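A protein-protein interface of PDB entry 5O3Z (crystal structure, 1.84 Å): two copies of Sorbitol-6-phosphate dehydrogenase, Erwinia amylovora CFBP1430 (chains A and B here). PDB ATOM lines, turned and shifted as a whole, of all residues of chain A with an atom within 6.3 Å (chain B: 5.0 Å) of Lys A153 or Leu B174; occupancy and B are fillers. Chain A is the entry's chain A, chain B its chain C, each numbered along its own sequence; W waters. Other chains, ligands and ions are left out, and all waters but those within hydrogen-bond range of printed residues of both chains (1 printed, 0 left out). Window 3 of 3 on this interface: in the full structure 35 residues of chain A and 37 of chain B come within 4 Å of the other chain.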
ATOM      1  N   ALA A  98      10.608  14.372 -18.585  1.00  0.00           N
ATOM      2  CA  ALA A  98      11.841  13.649 -18.517  1.00  0.00           C
ATOM      3  C   ALA A  98      11.623  12.252 -17.964  1.00  0.00           C
ATOM      4  O   ALA A  98      10.935  12.084 -16.951  1.00  0.00           O
ATOM      5  CB  ALA A  98      12.820  14.383 -17.606  1.00  0.00           C
ATOM      6  N   ALA A  99      12.255  11.274 -18.618  1.00  0.00           N
ATOM      7  CA  ALA A  99      12.316   9.881 -18.181  1.00  0.00           C
ATOM      8  C   ALA A  99      13.238   9.170 -19.169  1.00  0.00           C
ATOM      9  O   ALA A  99      13.143   9.442 -20.391  1.00  0.00           O
ATOM     10  CB  ALA A  99      10.938   9.220 -18.228  1.00  0.00           C
ATOM     11  N   VAL A 150      20.544  20.066 -30.061  1.00  0.00           N
ATOM     12  CA  VAL A 150      21.194  18.938 -29.416  1.00  0.00           C
ATOM     13  C   VAL A 150      20.180  18.108 -28.624  1.00  0.00           C
ATOM     14  O   VAL A 150      19.419  18.615 -27.798  1.00  0.00           O
ATOM     15  CB  VAL A 150      22.326  19.390 -28.477  1.00  0.00           C
ATOM     16  CG1 VAL A 150      23.276  20.169 -29.258  1.00  0.00           C
ATOM     17  CG2 VAL A 150      21.898  20.311 -27.402  1.00  0.00           C
ATOM     18  N   GLY A 151      20.201  16.800 -28.871  1.00  0.00           N
ATOM     19  CA  GLY A 151      19.311  15.865 -28.252  1.00  0.00           C
ATOM     20  C   GLY A 151      19.546  15.871 -26.740  1.00  0.00           C
ATOM     21  O   GLY A 151      20.609  16.273 -26.279  1.00  0.00           O
ATOM     22  N   SER A 152      18.506  15.563 -25.991  1.00  0.00           N
ATOM     23  CA  SER A 152      18.492  15.727 -24.524  1.00  0.00           C
ATOM     24  C   SER A 152      18.330  14.371 -23.914  1.00  0.00           C
ATOM     25  O   SER A 152      17.499  13.569 -24.347  1.00  0.00           O
ATOM     26  CB  SER A 152      17.372  16.692 -24.098  1.00  0.00           C
ATOM     27  OG  SER A 152      17.350  16.785 -22.673  1.00  0.00           O
ATOM     28  N   LYS A 153      19.229  14.059 -23.003  1.00  0.00           N
ATOM     29  CA  LYS A 153      19.217  12.835 -22.254  1.00  0.00           C
ATOM     30  C   LYS A 153      17.928  12.825 -21.446  1.00  0.00           C
ATOM     31  O   LYS A 153      17.569  13.858 -20.921  1.00  0.00           O
ATOM     32  CB  LYS A 153      20.431  12.806 -21.330  1.00  0.00           C
ATOM     33  CG  LYS A 153      20.631  11.500 -20.592  1.00  0.00           C
ATOM     34  CD  LYS A 153      21.978  11.442 -19.911  1.00  0.00           C
ATOM     35  CE  LYS A 153      22.242  10.029 -19.489  1.00  0.00           C
ATOM     36  NZ  LYS A 153      23.443   9.905 -18.607  1.00  0.00           N
ATOM     37  N   HIS A 154      17.194  11.719 -21.449  1.00  0.00           N
ATOM     38  CA  HIS A 154      15.885  11.573 -20.734  1.00  0.00           C
ATOM     39  C   HIS A 154      14.744  12.456 -21.252  1.00  0.00           C
ATOM     40  O   HIS A 154      13.725  12.582 -20.630  1.00  0.00           O
ATOM     41  CB  HIS A 154      16.066  11.719 -19.207  1.00  0.00           C
ATOM     42  CG  HIS A 154      17.054  10.743 -18.632  1.00  0.00           C
ATOM     43  ND1 HIS A 154      17.489  10.780 -17.317  1.00  0.00           N
ATOM     44  CD2 HIS A 154      17.684   9.681 -19.197  1.00  0.00           C
ATOM     45  CE1 HIS A 154      18.344   9.794 -17.099  1.00  0.00           C
ATOM     46  NE2 HIS A 154      18.466   9.099 -18.219  1.00  0.00           N
ATOM     47  N   ASN A 155      14.908  13.037 -22.421  1.00  0.00           N
ATOM     48  CA  ASN A 155      13.951  13.949 -22.934  1.00  0.00           C
ATOM     49  C   ASN A 155      13.667  13.700 -24.369  1.00  0.00           C
ATOM     50  O   ASN A 155      13.473  14.636 -25.129  1.00  0.00           O
ATOM     51  CB  ASN A 155      14.474  15.367 -22.702  1.00  0.00           C
ATOM     52  CG  ASN A 155      14.209  15.842 -21.295  1.00  0.00           C
ATOM     53  OD1 ASN A 155      13.071  16.185 -20.978  1.00  0.00           O
ATOM     54  ND2 ASN A 155      15.236  15.810 -20.427  1.00  0.00           N
ATOM     55  N   SER A 156      13.578  12.418 -24.723  1.00  0.00           N
ATOM     56  CA  SER A 156      13.338  11.996 -26.101  1.00  0.00           C
ATOM     57  C   SER A 156      12.134  12.630 -26.784  1.00  0.00           C
ATOM     58  O   SER A 156      12.216  13.015 -27.955  1.00  0.00           O
ATOM     59  CB  SER A 156      13.319  10.455 -26.191  1.00  0.00           C
ATOM     60  OG  SER A 156      12.143   9.899 -25.606  1.00  0.00           O
ATOM     61  N   SER A 159      12.987  16.355 -27.467  1.00  0.00           N
ATOM     62  CA  SER A 159      13.930  16.549 -28.575  1.00  0.00           C
ATOM     63  C   SER A 159      13.393  16.183 -29.956  1.00  0.00           C
ATOM     64  O   SER A 159      13.580  16.903 -30.907  1.00  0.00           O
ATOM     65  CB  SER A 159      15.235  15.824 -28.322  1.00  0.00           C
ATOM     66  OG  SER A 159      16.002  16.535 -27.340  1.00  0.00           O
ATOM     67  N   GLN B 170      19.624  11.142 -31.413  1.00  0.00           N
ATOM     68  CA  GLN B 170      20.551  11.711 -30.471  1.00  0.00           C
ATOM     69  C   GLN B 170      20.090  11.487 -28.993  1.00  0.00           C
ATOM     70  O   GLN B 170      20.942  11.227 -28.153  1.00  0.00           O
ATOM     71  CB  GLN B 170      20.746  13.184 -30.695  1.00  0.00           C
ATOM     72  CG  GLN B 170      21.338  13.592 -32.038  1.00  0.00           C
ATOM     73  CD  GLN B 170      21.675  15.047 -32.131  1.00  0.00           C
ATOM     74  OE1 GLN B 170      21.819  15.796 -31.103  1.00  0.00           O
ATOM     75  NE2 GLN B 170      21.939  15.473 -33.386  1.00  0.00           N
ATOM     76  N   SER B 171      18.795  11.685 -28.663  1.00  0.00           N
ATOM     77  CA  SER B 171      18.303  11.394 -27.257  1.00  0.00           C
ATOM     78  C   SER B 171      18.477   9.946 -26.865  1.00  0.00           C
ATOM     79  O   SER B 171      18.933   9.633 -25.762  1.00  0.00           O
ATOM     80  CB  SER B 171      16.869  11.808 -26.997  1.00  0.00           C
ATOM     81  OG  SER B 171      16.758  13.211 -27.012  1.00  0.00           O
ATOM     82  N   LEU B 172      18.206   9.038 -27.798  1.00  0.00           N
ATOM     83  CA  LEU B 172      18.379   7.599 -27.568  1.00  0.00           C
ATOM     84  C   LEU B 172      19.833   7.257 -27.320  1.00  0.00           C
ATOM     85  O   LEU B 172      20.181   6.480 -26.410  1.00  0.00           O
ATOM     86  CB  LEU B 172      17.895   6.844 -28.830  1.00  0.00           C
ATOM     87  CG  LEU B 172      16.443   6.708 -29.147  1.00  0.00           C
ATOM     88  CD1 LEU B 172      16.133   5.974 -30.457  1.00  0.00           C
ATOM     89  CD2 LEU B 172      15.709   6.000 -27.991  1.00  0.00           C
ATOM     90  N   ALA B 173      20.716   7.899 -28.098  1.00  0.00           N
ATOM     91  CA  ALA B 173      22.167   7.644 -27.959  1.00  0.00           C
ATOM     92  C   ALA B 173      22.643   8.052 -26.579  1.00  0.00           C
ATOM     93  O   ALA B 173      23.442   7.361 -25.962  1.00  0.00           O
ATOM     94  CB  ALA B 173      22.956   8.393 -29.054  1.00  0.00           C
ATOM     95  N   LEU B 174      22.143   9.190 -26.100  1.00  0.00           N
ATOM     96  CA  LEU B 174      22.567   9.701 -24.826  1.00  0.00           C
ATOM     97  C   LEU B 174      22.021   8.784 -23.724  1.00  0.00           C
ATOM     98  O   LEU B 174      22.761   8.488 -22.805  1.00  0.00           O
ATOM     99  CB  LEU B 174      22.128  11.140 -24.664  1.00  0.00           C
ATOM    100  CG  LEU B 174      22.867  12.202 -25.494  1.00  0.00           C
ATOM    101  CD1 LEU B 174      22.197  13.537 -25.453  1.00  0.00           C
ATOM    102  CD2 LEU B 174      24.340  12.339 -25.123  1.00  0.00           C
ATOM    103  N   ASP B 175      20.774   8.322 -23.845  1.00  0.00           N
ATOM    104  CA  ASP B 175      20.143   7.465 -22.830  1.00  0.00           C
ATOM    105  C   ASP B 175      20.782   6.086 -22.829  1.00  0.00           C
ATOM    106  O   ASP B 175      20.908   5.432 -21.800  1.00  0.00           O
ATOM    107  CB  ASP B 175      18.647   7.282 -23.105  1.00  0.00           C
ATOM    108  CG  ASP B 175      17.830   8.451 -22.682  1.00  0.00           C
ATOM    109  OD1 ASP B 175      18.417   9.556 -22.467  1.00  0.00           O
ATOM    110  OD2 ASP B 175      16.579   8.316 -22.573  1.00  0.00           O
ATOM    111  N   LEU B 176      21.197   5.625 -23.994  1.00  0.00           N
ATOM    112  CA  LEU B 176      21.614   4.228 -24.085  1.00  0.00           C
ATOM    113  C   LEU B 176      23.085   4.020 -24.028  1.00  0.00           C
ATOM    114  O   LEU B 176      23.531   2.886 -23.997  1.00  0.00           O
ATOM    115  CB  LEU B 176      21.047   3.558 -25.336  1.00  0.00           C
ATOM    116  CG  LEU B 176      19.513   3.525 -25.418  1.00  0.00           C
ATOM    117  CD1 LEU B 176      19.091   3.066 -26.818  1.00  0.00           C
ATOM    118  CD2 LEU B 176      18.956   2.637 -24.334  1.00  0.00           C
ATOM    119  N   ALA B 177      23.852   5.085 -24.029  1.00  0.00           N
ATOM    120  CA  ALA B 177      25.362   4.940 -24.127  1.00  0.00           C
ATOM    121  C   ALA B 177      25.986   4.159 -22.952  1.00  0.00           C
ATOM    122  O   ALA B 177      27.038   3.453 -23.065  1.00  0.00           O
ATOM    123  CB  ALA B 177      25.959   6.311 -24.225  1.00  0.00           C
ATOM    124  N   GLU B 178      25.372   4.312 -21.785  1.00  0.00           N
ATOM    125  CA  GLU B 178      25.877   3.634 -20.600  1.00  0.00           C
ATOM    126  C   GLU B 178      25.738   2.111 -20.716  1.00  0.00           C
ATOM    127  O   GLU B 178      26.332   1.371 -19.937  1.00  0.00           O
ATOM    128  CB  GLU B 178      25.136   4.107 -19.349  1.00  0.00           C
ATOM    129  CG  GLU B 178      23.673   3.696 -19.323  1.00  0.00           C
ATOM    130  CD  GLU B 178      22.878   4.384 -18.216  1.00  0.00           C
ATOM    131  OE1 GLU B 178      22.737   3.753 -17.152  1.00  0.00           O
ATOM    132  OE2 GLU B 178      22.423   5.541 -18.412  1.00  0.00           O
HETATM  133  O   HOH W   1      14.213   9.930 -23.159  1.00  0.00           O
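Water W1 lies within hydrogen-bond range of OD2 of Asp B175 (2.9 Å), O of Ala A99 (3.0 Å), N of Ser A156 (3.0 Å) and N of Asn A155 (3.3 Å).
The backbone carbonyl oxygen (O) of Ser A152 sits at hydrogen-bond distance from the side-chain hydroxyl (OG) of Ser B171 (2.8 Å).
The backbone NH (N) of Gly A151 lies within hydrogen-bond range of the side-chain amide oxygen (OE1) of Gln B170 (2.9 Å).
OD1 of Asp B175 lies within hydrogen-bond range of N of His A154 (2.7 Å).
The side-chain hydroxyl (OG) of Ser A159 lies close to the side-chain hydroxyl (OG) of Ser B171 (3.4 Å).
No position is printed for both chains.
Of the 9 printed residues of chain B, 4 touch a printed residue of chain A.
Hydrophobic or aromatic side chains of chain B within 4 Å of the printed part of chain A: Leu B174.
Among the printed residues, 10 pairs touch across the chains.
Among the printed residues, no Asp or Glu carboxylate lies within 4 Å of a Lys or Arg side-chain nitrogen of the other chain.
Gln B170 touches Val A150 (OE1 to CA, 3.6 Å).
Gly A151 touches Ser B171 (C to OG, 3.9 Å).
Gly A151 touches Leu B174 (O to CD1, 3.3 Å).
Leu B174 touches Lys A153.
Asp B175 touches Lys A153 (OD1 to CA, 3.4 Å).
CA of Ser A156 touches CB of Ser B171, 3.6 Å away.
N of Ala A99 sits at hydrogen-bond distance from O of His A154, at 2.8 Å.
ND2 of Asn A155 sits at hydrogen-bond distance from O of Lys A153 (3.1 Å).
ND2 of Asn A155 lies close to OG of Ser A152, at 3.2 Å.
The backbone NH (N) of Ser A152 is in hydrogen-bond range of the side-chain hydroxyl (OG) of Ser A159 (3.0 Å).
Of chain A, only Gly A151 (3.3 Å) and Lys A153 (3.7 Å) come within 4 Å of Leu B174.
Of the printed residues of chain A, Gln B170 touches Val A150 and Gly A151.
Printed residues of chain B within 4 Å of His A154: Asp B175 (2.7 Å).
Of the printed residues of chain B, Ser A156 touches Ser B171.
Printed residues of chain B within 4 Å of Ser A159: Ser B171.
The nearest residue of chain A that does not touch Leu B174 is Ser A152 (4.2 Å).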
